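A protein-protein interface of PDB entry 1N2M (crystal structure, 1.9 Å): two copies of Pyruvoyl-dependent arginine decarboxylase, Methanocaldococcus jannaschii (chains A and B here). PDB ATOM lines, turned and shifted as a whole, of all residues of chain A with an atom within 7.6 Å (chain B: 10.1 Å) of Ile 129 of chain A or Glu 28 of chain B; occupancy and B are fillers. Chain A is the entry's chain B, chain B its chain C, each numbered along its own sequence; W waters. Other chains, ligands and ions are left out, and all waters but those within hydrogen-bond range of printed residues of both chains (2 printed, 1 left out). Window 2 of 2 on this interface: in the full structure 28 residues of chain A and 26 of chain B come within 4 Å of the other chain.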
ATOM      1  N   ALA A  96      21.267   4.110   6.959  1.00  0.00           N
ATOM      2  CA  ALA A  96      22.034   3.439   7.990  1.00  0.00           C
ATOM      3  C   ALA A  96      22.395   4.506   9.003  1.00  0.00           C
ATOM      4  O   ALA A  96      23.023   5.509   8.659  1.00  0.00           O
ATOM      5  CB  ALA A  96      23.289   2.819   7.396  1.00  0.00           C
ATOM      6  N   LEU A 106      24.026   7.046   6.316  1.00  0.00           N
ATOM      7  CA  LEU A 106      24.198   6.775   4.895  1.00  0.00           C
ATOM      8  C   LEU A 106      22.861   6.426   4.258  1.00  0.00           C
ATOM      9  O   LEU A 106      22.155   5.533   4.723  1.00  0.00           O
ATOM     10  CB  LEU A 106      25.180   5.625   4.679  1.00  0.00           C
ATOM     11  CG  LEU A 106      25.454   5.281   3.215  1.00  0.00           C
ATOM     12  CD1 LEU A 106      26.189   6.420   2.521  1.00  0.00           C
ATOM     13  CD2 LEU A 106      26.261   4.011   3.142  1.00  0.00           C
ATOM     14  N   MET A 108      20.874   5.060   1.026  1.00  0.00           N
ATOM     15  CA  MET A 108      21.030   4.269  -0.181  1.00  0.00           C
ATOM     16  C   MET A 108      19.675   4.145  -0.847  1.00  0.00           C
ATOM     17  O   MET A 108      18.639   4.137  -0.182  1.00  0.00           O
ATOM     18  CB  MET A 108      21.565   2.869   0.145  1.00  0.00           C
ATOM     19  CG  MET A 108      23.036   2.828   0.470  1.00  0.00           C
ATOM     20  SD  MET A 108      24.005   3.227  -0.984  1.00  0.00           S
ATOM     21  CE  MET A 108      25.637   3.315  -0.304  1.00  0.00           C
ATOM     22  N   THR A 122      17.960  -5.717  -0.612  1.00  0.00           N
ATOM     23  CA  THR A 122      19.101  -5.210  -1.363  1.00  0.00           C
ATOM     24  C   THR A 122      19.534  -3.826  -0.896  1.00  0.00           C
ATOM     25  O   THR A 122      20.723  -3.580  -0.693  1.00  0.00           O
ATOM     26  CB  THR A 122      18.783  -5.135  -2.870  1.00  0.00           C
ATOM     27  OG1 THR A 122      18.382  -6.427  -3.333  1.00  0.00           O
ATOM     28  CG2 THR A 122      20.007  -4.674  -3.661  1.00  0.00           C
ATOM     29  N   VAL A 123      18.569  -2.926  -0.723  1.00  0.00           N
ATOM     30  CA  VAL A 123      18.883  -1.568  -0.302  1.00  0.00           C
ATOM     31  C   VAL A 123      19.412  -1.493   1.131  1.00  0.00           C
ATOM     32  O   VAL A 123      20.187  -0.591   1.459  1.00  0.00           O
ATOM     33  CB  VAL A 123      17.682  -0.614  -0.503  1.00  0.00           C
ATOM     34  CG1 VAL A 123      16.729  -0.677   0.689  1.00  0.00           C
ATOM     35  CG2 VAL A 123      18.181   0.812  -0.757  1.00  0.00           C
ATOM     36  N   ARG A 124      19.002  -2.435   1.983  1.00  0.00           N
ATOM     37  CA  ARG A 124      19.482  -2.459   3.366  1.00  0.00           C
ATOM     38  C   ARG A 124      20.939  -2.909   3.378  1.00  0.00           C
ATOM     39  O   ARG A 124      21.772  -2.334   4.082  1.00  0.00           O
ATOM     40  CB  ARG A 124      18.637  -3.394   4.240  1.00  0.00           C
ATOM     41  CG  ARG A 124      17.224  -2.893   4.509  1.00  0.00           C
ATOM     42  CD  ARG A 124      16.429  -3.892   5.351  1.00  0.00           C
ATOM     43  NE  ARG A 124      16.973  -4.027   6.704  1.00  0.00           N
ATOM     44  CZ  ARG A 124      16.720  -3.183   7.698  1.00  0.00           C
ATOM     45  NH1 ARG A 124      15.926  -2.135   7.501  1.00  0.00           N
ATOM     46  NH2 ARG A 124      17.275  -3.377   8.887  1.00  0.00           N
ATOM     47  N   GLU A 125      21.248  -3.913   2.561  1.00  0.00           N
ATOM     48  CA  GLU A 125      22.608  -4.426   2.472  1.00  0.00           C
ATOM     49  C   GLU A 125      23.535  -3.355   1.901  1.00  0.00           C
ATOM     50  O   GLU A 125      24.677  -3.240   2.321  1.00  0.00           O
ATOM     51  CB  GLU A 125      22.656  -5.692   1.612  1.00  0.00           C
ATOM     52  CG  GLU A 125      24.018  -6.396   1.597  1.00  0.00           C
ATOM     53  CD  GLU A 125      24.507  -6.811   2.986  1.00  0.00           C
ATOM     54  OE1 GLU A 125      23.669  -7.125   3.862  1.00  0.00           O
ATOM     55  OE2 GLU A 125      25.740  -6.829   3.201  1.00  0.00           O
ATOM     56  N   MET A 126      23.025  -2.549   0.972  1.00  0.00           N
ATOM     57  CA  MET A 126      23.824  -1.476   0.366  1.00  0.00           C
ATOM     58  C   MET A 126      24.220  -0.448   1.426  1.00  0.00           C
ATOM     59  O   MET A 126      25.346   0.048   1.428  1.00  0.00           O
ATOM     60  CB  MET A 126      23.042  -0.796  -0.755  1.00  0.00           C
ATOM     61  CG  MET A 126      22.825  -1.668  -1.980  1.00  0.00           C
ATOM     62  SD  MET A 126      21.625  -0.978  -3.128  1.00  0.00           S
ATOM     63  CE  MET A 126      22.503   0.448  -3.713  1.00  0.00           C
ATOM     64  N   ALA A 127      23.293  -0.141   2.328  1.00  0.00           N
ATOM     65  CA  ALA A 127      23.563   0.812   3.402  1.00  0.00           C
ATOM     66  C   ALA A 127      24.581   0.204   4.367  1.00  0.00           C
ATOM     67  O   ALA A 127      25.521   0.872   4.801  1.00  0.00           O
ATOM     68  CB  ALA A 127      22.272   1.160   4.139  1.00  0.00           C
ATOM     69  N   LYS A 128      24.414  -1.082   4.664  1.00  0.00           N
ATOM     70  CA  LYS A 128      25.325  -1.776   5.570  1.00  0.00           C
ATOM     71  C   LYS A 128      26.733  -1.783   4.982  1.00  0.00           C
ATOM     72  O   LYS A 128      27.708  -1.522   5.685  1.00  0.00           O
ATOM     73  CB  LYS A 128      24.849  -3.207   5.822  1.00  0.00           C
ATOM     74  CG  LYS A 128      25.551  -3.892   6.988  1.00  0.00           C
ATOM     75  CD  LYS A 128      25.070  -5.322   7.150  1.00  0.00           C
ATOM     76  CE  LYS A 128      25.704  -5.985   8.361  1.00  0.00           C
ATOM     77  NZ  LYS A 128      25.446  -7.450   8.371  1.00  0.00           N
ATOM     78  N   ILE A 129      26.826  -2.052   3.684  1.00  0.00           N
ATOM     79  CA  ILE A 129      28.110  -2.070   2.985  1.00  0.00           C
ATOM     80  C   ILE A 129      28.784  -0.705   3.067  1.00  0.00           C
ATOM     81  O   ILE A 129      29.989  -0.621   3.296  1.00  0.00           O
ATOM     82  CB  ILE A 129      27.933  -2.444   1.498  1.00  0.00           C
ATOM     83  CG1 ILE A 129      27.539  -3.913   1.371  1.00  0.00           C
ATOM     84  CG2 ILE A 129      29.219  -2.175   0.716  1.00  0.00           C
ATOM     85  CD1 ILE A 129      27.029  -4.278  -0.004  1.00  0.00           C
ATOM     86  N   GLY A 130      28.003   0.360   2.889  1.00  0.00           N
ATOM     87  CA  GLY A 130      28.561   1.700   2.950  1.00  0.00           C
ATOM     88  C   GLY A 130      29.229   1.936   4.288  1.00  0.00           C
ATOM     89  O   GLY A 130      30.301   2.547   4.368  1.00  0.00           O
ATOM     90  N   PHE A 131      28.576   1.465   5.346  1.00  0.00           N
ATOM     91  CA  PHE A 131      29.106   1.590   6.696  1.00  0.00           C
ATOM     92  C   PHE A 131      30.351   0.728   6.862  1.00  0.00           C
ATOM     93  O   PHE A 131      31.289   1.115   7.551  1.00  0.00           O
ATOM     94  CB  PHE A 131      28.043   1.202   7.723  1.00  0.00           C
ATOM     95  CG  PHE A 131      27.337   2.375   8.327  1.00  0.00           C
ATOM     96  CD1 PHE A 131      26.958   3.458   7.541  1.00  0.00           C
ATOM     97  CD2 PHE A 131      27.070   2.413   9.686  1.00  0.00           C
ATOM     98  CE1 PHE A 131      26.322   4.568   8.104  1.00  0.00           C
ATOM     99  CE2 PHE A 131      26.435   3.516  10.257  1.00  0.00           C
ATOM    100  CZ  PHE A 131      26.061   4.596   9.462  1.00  0.00           C
ATOM    101  N   GLU A 132      30.353  -0.436   6.219  1.00  0.00           N
ATOM    102  CA  GLU A 132      31.491  -1.354   6.262  1.00  0.00           C
ATOM    103  C   GLU A 132      32.702  -0.702   5.583  1.00  0.00           C
ATOM    104  O   GLU A 132      33.826  -0.789   6.083  1.00  0.00           O
ATOM    105  CB  GLU A 132      31.136  -2.664   5.549  1.00  0.00           C
ATOM    106  CG  GLU A 132      32.274  -3.679   5.472  1.00  0.00           C
ATOM    107  CD  GLU A 132      31.934  -4.906   4.627  1.00  0.00           C
ATOM    108  OE1 GLU A 132      30.883  -4.909   3.945  1.00  0.00           O
ATOM    109  OE2 GLU A 132      32.734  -5.870   4.640  1.00  0.00           O
ATOM    110  N   MET A 133      32.454  -0.027   4.462  1.00  0.00           N
ATOM    111  CA  MET A 133      33.507   0.654   3.712  1.00  0.00           C
ATOM    112  C   MET A 133      34.109   1.797   4.524  1.00  0.00           C
ATOM    113  O   MET A 133      35.278   2.143   4.356  1.00  0.00           O
ATOM    114  CB  MET A 133      32.958   1.193   2.388  1.00  0.00           C
ATOM    115  CG  MET A 133      32.662   0.115   1.352  1.00  0.00           C
ATOM    116  SD  MET A 133      31.856   0.749  -0.139  1.00  0.00           S
ATOM    117  CE  MET A 133      33.267   1.001  -1.245  1.00  0.00           C
ATOM    118  N   ARG A 134      33.303   2.380   5.405  1.00  0.00           N
ATOM    119  CA  ARG A 134      33.753   3.483   6.246  1.00  0.00           C
ATOM    120  C   ARG A 134      34.317   2.994   7.576  1.00  0.00           C
ATOM    121  O   ARG A 134      35.096   3.698   8.221  1.00  0.00           O
ATOM    122  CB  ARG A 134      32.600   4.457   6.506  1.00  0.00           C
ATOM    123  CG  ARG A 134      32.151   5.240   5.281  1.00  0.00           C
ATOM    124  CD  ARG A 134      30.890   6.025   5.570  1.00  0.00           C
ATOM    125  NE  ARG A 134      30.551   6.960   4.497  1.00  0.00           N
ATOM    126  CZ  ARG A 134      30.102   6.602   3.297  1.00  0.00           C
ATOM    127  NH1 ARG A 134      29.931   5.319   3.001  1.00  0.00           N
ATOM    128  NH2 ARG A 134      29.820   7.530   2.394  1.00  0.00           N
ATOM    129  N   GLY A 135      33.941   1.776   7.964  1.00  0.00           N
ATOM    130  CA  GLY A 135      34.395   1.218   9.224  1.00  0.00           C
ATOM    131  C   GLY A 135      33.585   1.804  10.366  1.00  0.00           C
ATOM    132  O   GLY A 135      34.058   1.910  11.499  1.00  0.00           O
ATOM    133  N   LEU A 138      27.255   0.339  13.230  1.00  0.00           N
ATOM    134  CA  LEU A 138      25.846   0.504  12.911  1.00  0.00           C
ATOM    135  C   LEU A 138      24.906   0.500  14.116  1.00  0.00           C
ATOM    136  O   LEU A 138      25.031  -0.337  15.014  1.00  0.00           O
ATOM    137  CB  LEU A 138      25.429  -0.618  11.954  1.00  0.00           C
ATOM    138  CG  LEU A 138      24.035  -0.625  11.336  1.00  0.00           C
ATOM    139  CD1 LEU A 138      23.893   0.564  10.398  1.00  0.00           C
ATOM    140  CD2 LEU A 138      23.831  -1.931  10.574  1.00  0.00           C
ATOM    141  N   ILE A 141      19.362   0.130  10.579  1.00  0.00           N
ATOM    142  CA  ILE A 141      19.077   0.529   9.221  1.00  0.00           C
ATOM    143  C   ILE A 141      17.570   0.608   9.102  1.00  0.00           C
ATOM    144  O   ILE A 141      16.865  -0.338   9.461  1.00  0.00           O
ATOM    145  CB  ILE A 141      19.611  -0.493   8.209  1.00  0.00           C
ATOM    146  CG1 ILE A 141      21.142  -0.536   8.269  1.00  0.00           C
ATOM    147  CG2 ILE A 141      19.143  -0.120   6.793  1.00  0.00           C
ATOM    148  CD1 ILE A 141      21.759  -1.646   7.429  1.00  0.00           C
ATOM    149  N   SER B  25      36.655   3.704  -7.413  1.00  0.00           N
ATOM    150  CA  SER B  25      36.468   2.638  -6.453  1.00  0.00           C
ATOM    151  C   SER B  25      35.635   1.507  -7.001  1.00  0.00           C
ATOM    152  O   SER B  25      34.818   1.689  -7.907  1.00  0.00           O
ATOM    153  CB  SER B  25      35.786   3.183  -5.197  1.00  0.00           C
ATOM    154  OG  SER B  25      35.424   2.148  -4.300  1.00  0.00           O
ATOM    155  N   GLU B  26      35.901   0.322  -6.471  1.00  0.00           N
ATOM    156  CA  GLU B  26      35.140  -0.861  -6.811  1.00  0.00           C
ATOM    157  C   GLU B  26      33.954  -0.802  -5.851  1.00  0.00           C
ATOM    158  O   GLU B  26      33.978  -0.053  -4.870  1.00  0.00           O
ATOM    159  CB  GLU B  26      35.958  -2.126  -6.528  1.00  0.00           C
ATOM    160  CG  GLU B  26      37.033  -2.436  -7.562  1.00  0.00           C
ATOM    161  CD  GLU B  26      36.446  -2.886  -8.885  1.00  0.00           C
ATOM    162  OE1 GLU B  26      36.766  -2.268  -9.922  1.00  0.00           O
ATOM    163  OE2 GLU B  26      35.659  -3.857  -8.890  1.00  0.00           O
ATOM    164  N   GLY B  27      32.923  -1.587  -6.126  1.00  0.00           N
ATOM    165  CA  GLY B  27      31.768  -1.599  -5.254  1.00  0.00           C
ATOM    166  C   GLY B  27      30.902  -2.807  -5.522  1.00  0.00           C
ATOM    167  O   GLY B  27      30.957  -3.384  -6.608  1.00  0.00           O
ATOM    168  N   GLU B  28      30.110  -3.200  -4.531  1.00  0.00           N
ATOM    169  CA  GLU B  28      29.227  -4.348  -4.689  1.00  0.00           C
ATOM    170  C   GLU B  28      27.998  -4.024  -5.538  1.00  0.00           C
ATOM    171  O   GLU B  28      27.310  -4.924  -6.015  1.00  0.00           O
ATOM    172  CB  GLU B  28      28.837  -4.915  -3.321  1.00  0.00           C
ATOM    173  CG  GLU B  28      30.001  -5.595  -2.606  1.00  0.00           C
ATOM    174  CD  GLU B  28      29.600  -6.251  -1.294  1.00  0.00           C
ATOM    175  OE1 GLU B  28      30.109  -5.812  -0.238  1.00  0.00           O
ATOM    176  OE2 GLU B  28      28.790  -7.209  -1.315  1.00  0.00           O
ATOM    177  N   THR B  29      27.707  -2.735  -5.690  1.00  0.00           N
ATOM    178  CA  THR B  29      26.590  -2.265  -6.504  1.00  0.00           C
ATOM    179  C   THR B  29      27.043  -0.961  -7.150  1.00  0.00           C
ATOM    180  O   THR B  29      28.077  -0.402  -6.779  1.00  0.00           O
ATOM    181  CB  THR B  29      25.316  -1.952  -5.675  1.00  0.00           C
ATOM    182  OG1 THR B  29      25.565  -0.843  -4.802  1.00  0.00           O
ATOM    183  CG2 THR B  29      24.869  -3.164  -4.875  1.00  0.00           C
ATOM    184  N   PRO B  30      26.310  -0.491  -8.162  1.00  0.00           N
ATOM    185  CA  PRO B  30      26.707   0.763  -8.806  1.00  0.00           C
ATOM    186  C   PRO B  30      26.736   1.929  -7.812  1.00  0.00           C
ATOM    187  O   PRO B  30      27.681   2.715  -7.807  1.00  0.00           O
ATOM    188  CB  PRO B  30      25.636   0.940  -9.878  1.00  0.00           C
ATOM    189  CG  PRO B  30      25.354  -0.471 -10.276  1.00  0.00           C
ATOM    190  CD  PRO B  30      25.259  -1.170  -8.941  1.00  0.00           C
ATOM    191  N   LEU B  31      25.742   2.000  -6.928  1.00  0.00           N
ATOM    192  CA  LEU B  31      25.699   3.085  -5.951  1.00  0.00           C
ATOM    193  C   LEU B  31      26.801   2.953  -4.895  1.00  0.00           C
ATOM    194  O   LEU B  31      27.363   3.957  -4.462  1.00  0.00           O
ATOM    195  CB  LEU B  31      24.316   3.187  -5.303  1.00  0.00           C
ATOM    196  CG  LEU B  31      24.077   4.418  -4.418  1.00  0.00           C
ATOM    197  CD1 LEU B  31      24.335   5.717  -5.188  1.00  0.00           C
ATOM    198  CD2 LEU B  31      22.658   4.385  -3.896  1.00  0.00           C
ATOM    199  N   ASN B  32      27.132   1.723  -4.502  1.00  0.00           N
ATOM    200  CA  ASN B  32      28.205   1.515  -3.533  1.00  0.00           C
ATOM    201  C   ASN B  32      29.544   1.896  -4.171  1.00  0.00           C
ATOM    202  O   ASN B  32      30.428   2.429  -3.499  1.00  0.00           O
ATOM    203  CB  ASN B  32      28.245   0.066  -3.038  1.00  0.00           C
ATOM    204  CG  ASN B  32      27.117  -0.258  -2.072  1.00  0.00           C
ATOM    205  OD1 ASN B  32      27.029   0.302  -0.975  1.00  0.00           O
ATOM    206  ND2 ASN B  32      26.260  -1.179  -2.468  1.00  0.00           N
ATOM    207  N   ALA B  33      29.690   1.615  -5.466  1.00  0.00           N
ATOM    208  CA  ALA B  33      30.913   1.966  -6.193  1.00  0.00           C
ATOM    209  C   ALA B  33      30.984   3.487  -6.296  1.00  0.00           C
ATOM    210  O   ALA B  33      32.038   4.087  -6.081  1.00  0.00           O
ATOM    211  CB  ALA B  33      30.903   1.345  -7.581  1.00  0.00           C
ATOM    212  N   PHE B  34      29.849   4.107  -6.607  1.00  0.00           N
ATOM    213  CA  PHE B  34      29.774   5.559  -6.713  1.00  0.00           C
ATOM    214  C   PHE B  34      30.163   6.160  -5.363  1.00  0.00           C
ATOM    215  O   PHE B  34      31.014   7.048  -5.291  1.00  0.00           O
ATOM    216  CB  PHE B  34      28.360   5.988  -7.094  1.00  0.00           C
ATOM    217  CG  PHE B  34      28.190   7.476  -7.219  1.00  0.00           C
ATOM    218  CD1 PHE B  34      28.655   8.151  -8.340  1.00  0.00           C
ATOM    219  CD2 PHE B  34      27.562   8.202  -6.211  1.00  0.00           C
ATOM    220  CE1 PHE B  34      28.496   9.535  -8.458  1.00  0.00           C
ATOM    221  CE2 PHE B  34      27.399   9.579  -6.317  1.00  0.00           C
ATOM    222  CZ  PHE B  34      27.866  10.246  -7.442  1.00  0.00           C
ATOM    223  N   ASP B  35      29.558   5.630  -4.301  1.00  0.00           N
ATOM    224  CA  ASP B  35      29.814   6.061  -2.928  1.00  0.00           C
ATOM    225  C   ASP B  35      31.304   5.923  -2.616  1.00  0.00           C
ATOM    226  O   ASP B  35      31.926   6.850  -2.090  1.00  0.00           O
ATOM    227  CB  ASP B  35      28.986   5.207  -1.957  1.00  0.00           C
ATOM    228  CG  ASP B  35      29.115   5.654  -0.500  1.00  0.00           C
ATOM    229  OD1 ASP B  35      29.032   6.869  -0.220  1.00  0.00           O
ATOM    230  OD2 ASP B  35      29.264   4.777   0.374  1.00  0.00           O
ATOM    231  N   GLY B  36      31.873   4.774  -2.973  1.00  0.00           N
ATOM    232  CA  GLY B  36      33.286   4.538  -2.736  1.00  0.00           C
ATOM    233  C   GLY B  36      34.172   5.532  -3.472  1.00  0.00           C
ATOM    234  O   GLY B  36      35.213   5.939  -2.957  1.00  0.00           O
ATOM    235  N   ALA B  37      33.748   5.941  -4.668  1.00  0.00           N
ATOM    236  CA  ALA B  37      34.518   6.900  -5.462  1.00  0.00           C
ATOM    237  C   ALA B  37      34.511   8.287  -4.812  1.00  0.00           C
ATOM    238  O   ALA B  37      35.528   8.985  -4.819  1.00  0.00           O
ATOM    239  CB  ALA B  37      33.967   6.976  -6.873  1.00  0.00           C
ATOM    240  N   LEU B  39      34.223   8.942  -1.652  1.00  0.00           N
ATOM    241  CA  LEU B  39      35.104   8.788  -0.498  1.00  0.00           C
ATOM    242  C   LEU B  39      36.560   8.844  -0.938  1.00  0.00           C
ATOM    243  O   LEU B  39      37.387   9.498  -0.308  1.00  0.00           O
ATOM    244  CB  LEU B  39      34.835   7.452   0.186  1.00  0.00           C
ATOM    245  CG  LEU B  39      33.524   7.354   0.963  1.00  0.00           C
ATOM    246  CD1 LEU B  39      33.236   5.904   1.308  1.00  0.00           C
ATOM    247  CD2 LEU B  39      33.618   8.215   2.227  1.00  0.00           C
ATOM    248  N   ILE B  81      30.260   4.300 -14.490  1.00  0.00           N
ATOM    249  CA  ILE B  81      30.296   3.044 -13.770  1.00  0.00           C
ATOM    250  C   ILE B  81      30.302   1.934 -14.804  1.00  0.00           C
ATOM    251  O   ILE B  81      29.625   2.027 -15.829  1.00  0.00           O
ATOM    252  CB  ILE B  81      29.067   2.893 -12.854  1.00  0.00           C
ATOM    253  CG1 ILE B  81      29.010   4.065 -11.867  1.00  0.00           C
ATOM    254  CG2 ILE B  81      29.141   1.592 -12.087  1.00  0.00           C
ATOM    255  CD1 ILE B  81      27.788   4.058 -10.976  1.00  0.00           C
ATOM    256  N   SER B  82      31.109   0.912 -14.553  1.00  0.00           N
ATOM    257  CA  SER B  82      31.209  -0.218 -15.457  1.00  0.00           C
ATOM    258  C   SER B  82      31.397  -1.514 -14.689  1.00  0.00           C
ATOM    259  O   SER B  82      32.119  -1.559 -13.693  1.00  0.00           O
ATOM    260  CB  SER B  82      32.374  -0.029 -16.430  1.00  0.00           C
ATOM    261  OG  SER B  82      32.624  -1.222 -17.149  1.00  0.00           O
ATOM    262  N   ASP B  83      30.732  -2.560 -15.165  1.00  0.00           N
ATOM    263  CA  ASP B  83      30.818  -3.887 -14.562  1.00  0.00           C
ATOM    264  C   ASP B  83      31.505  -4.870 -15.517  1.00  0.00           C
ATOM    265  O   ASP B  83      31.251  -6.079 -15.477  1.00  0.00           O
ATOM    266  CB  ASP B  83      29.423  -4.394 -14.171  1.00  0.00           C
ATOM    267  CG  ASP B  83      28.440  -4.405 -15.339  1.00  0.00           C
ATOM    268  OD1 ASP B  83      28.833  -4.109 -16.486  1.00  0.00           O
ATOM    269  OD2 ASP B  83      27.257  -4.715 -15.103  1.00  0.00           O
ATOM    270  N   LYS B 152      35.605  -5.813 -11.005  1.00  0.00           N
ATOM    271  CA  LYS B 152      34.292  -6.445 -11.052  1.00  0.00           C
ATOM    272  C   LYS B 152      33.244  -5.384 -11.372  1.00  0.00           C
ATOM    273  O   LYS B 152      32.448  -5.533 -12.298  1.00  0.00           O
ATOM    274  CB  LYS B 152      33.962  -7.111  -9.714  1.00  0.00           C
ATOM    275  CG  LYS B 152      34.957  -8.178  -9.283  1.00  0.00           C
ATOM    276  CD  LYS B 152      34.470  -8.918  -8.045  1.00  0.00           C
ATOM    277  CE  LYS B 152      33.227  -9.743  -8.347  1.00  0.00           C
ATOM    278  NZ  LYS B 152      33.503 -10.788  -9.376  1.00  0.00           N
ATOM    279  N   LEU B 153      33.269  -4.298 -10.607  1.00  0.00           N
ATOM    280  CA  LEU B 153      32.328  -3.200 -10.786  1.00  0.00           C
ATOM    281  C   LEU B 153      33.003  -1.974 -10.205  1.00  0.00           C
ATOM    282  O   LEU B 153      33.237  -1.893  -8.996  1.00  0.00           O
ATOM    283  CB  LEU B 153      31.013  -3.505 -10.059  1.00  0.00           C
ATOM    284  CG  LEU B 153      29.899  -2.453 -10.029  1.00  0.00           C
ATOM    285  CD1 LEU B 153      29.579  -1.952 -11.416  1.00  0.00           C
ATOM    286  CD2 LEU B 153      28.666  -3.071  -9.394  1.00  0.00           C
ATOM    287  N   GLY B 154      33.354  -1.040 -11.083  1.00  0.00           N
ATOM    288  CA  GLY B 154      34.035   0.156 -10.633  1.00  0.00           C
ATOM    289  C   GLY B 154      33.411   1.446 -11.104  1.00  0.00           C
ATOM    290  O   GLY B 154      32.608   1.469 -12.035  1.00  0.00           O
ATOM    291  N   CYS B 155      33.802   2.533 -10.454  1.00  0.00           N
ATOM    292  CA  CYS B 155      33.296   3.847 -10.794  1.00  0.00           C
ATOM    293  C   CYS B 155      34.425   4.859 -10.797  1.00  0.00           C
ATOM    294  O   CYS B 155      35.246   4.877  -9.888  1.00  0.00           O
ATOM    295  CB  CYS B 155      32.238   4.282  -9.777  1.00  0.00           C
ATOM    296  SG  CYS B 155      31.784   6.030  -9.883  1.00  0.00           S
HETATM  297  O   HOH W   1      30.059  -6.955   2.238  1.00  0.00           O
HETATM  298  O   HOH W   2      30.894  -2.122  -2.123  1.00  0.00           O
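The side-chain amide oxygen (OD1) of Asn 32 of chain B sits close to the backbone carbonyl oxygen (O) of Met 126 of chain A (2.9 Å).
The guanidinium group of Arg 134 of chain A lies within salt-bridge range of the side-chain carboxylate of Asp 35 of chain B (2.8 Å).
The side-chain hydroxyl (OG1) of Thr 29 of chain B sits at hydrogen-bond distance from the side-chain amide nitrogen (ND2) of Asn 32 of chain B (2.5 Å).
O of Ser 25 of chain B sits at hydrogen-bond distance from N of Cys 155 of chain B (2.9 Å).
The backbone carbonyl oxygen (O) of Gly 130 of chain A is in hydrogen-bond range of the guanidinium group (NH1) of Arg 134 of chain A (3.1 Å).
The backbone NH (N) of Ala 96 of chain A lies within hydrogen-bond range of the backbone carbonyl oxygen (O) of Leu 106 of chain A, at 2.8 Å.
The side-chain carboxylate of Glu 26 of chain B lies within hydrogen-bond range of the backbone NH of Leu 153 of chain B, 3.0 Å away.
Among the printed residues, pairs that only touch across the chains: Leu 106 of chain A with Asp 35 of chain B, Met 108 of chain A with Leu 31 of chain B, Met 108 of chain A with Asn 32 of chain B, Met 108 of chain A with Asp 35 of chain B, Met 126 of chain A with Thr 29 of chain B, Met 126 of chain A with Leu 31 of chain B, Ile 129 of chain A with Glu 28 of chain B, Ile 129 of chain A with Asn 32 of chain B, Gly 130 of chain A with Asn 32 of chain B, Met 133 of chain A with Ser 25 of chain B, Met 133 of chain A with Glu 26 of chain B, Met 133 of chain A with Asn 32 of chain B, Met 133 of chain A with Gly 36 of chain B and Arg 134 of chain A with Leu 39 of chain B.
Of chain B, only Glu 28 (3.4 Å) and Asn 32 (3.7 Å) come within 4 Å of Ile 129 of chain A.
Of chain A, only Ile 129 (3.4 Å) comes within 4 Å of Glu 28 of chain B.
No residue of chain B comes within 4 Å of Ala 127 of chain A.
Of the printed residues of chain A, Leu 39 of chain B touches Arg 134 (3.8 Å).
Of the printed residues of chain A, Gly 36 of chain B touches Met 133.
Of the printed residues of chain B, Met 108 of chain A touches Leu 31, Asn 32 and Asp 35.
Of the printed residues of chain B, Met 133 of chain A touches Ser 25 (3.9 Å), Glu 26 (3.8 Å), Asn 32 (3.9 Å) and Gly 36 (3.8 Å).
Of the printed residues of chain A, Leu 31 of chain B touches Met 108 (3.4 Å) and Met 126 (3.6 Å).
The nearest residue of chain B that does not touch Ile 129 of chain A is Thr 29 of chain B (5.4 Å).
The nearest residue of chain A that does not touch Glu 28 of chain B is Glu 132 of chain A (4.3 Å).
Printed residues of chain A that touch a printed residue of chain B: Leu 106, Met 108, Met 126, Ile 129, Gly 130, Met 133 and Arg 134.
Hydrophobic or aromatic side chains of chain A within 4 Å of the printed part of chain B: Leu 106, Met 108, Met 126, Ile 129 and Met 133.
Of the 21 printed residues of chain B, 9 touch a printed residue of chain A.
Printed residues of chain B that touch a printed residue of chain A: Ser 25, Glu 26, Glu 28, Thr 29, Leu 31, Asn 32, Asp 35, Gly 36 and Leu 39.
Hydrophobic or aromatic side chains of chain B within 4 Å of the printed part of chain A: Leu 31 and Leu 39.
Among the printed residues, 16 pairs touch across the chains.
Among the printed residues, Asp or Glu carboxylates within 4 Å of a Lys or Arg side-chain nitrogen of the other chain: Arg 134 of chain A with Asp 35 of chain B.
No position is printed for both chains.
Of the 16 pairs that touch across the chains among the printed residues, none has its exchanged pair printed and touching as well.
Water W1 bridges the side-chain carboxylate (OE1) of Glu 28 of chain B (2.7 Å) and the side-chain carboxylate (OE1) of Glu 132 of chain A (2.8 Å).
Water W2 bridges N of Glu 28 of chain B (2.8 Å) and SD of Met 133 of chain A (3.6 Å).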
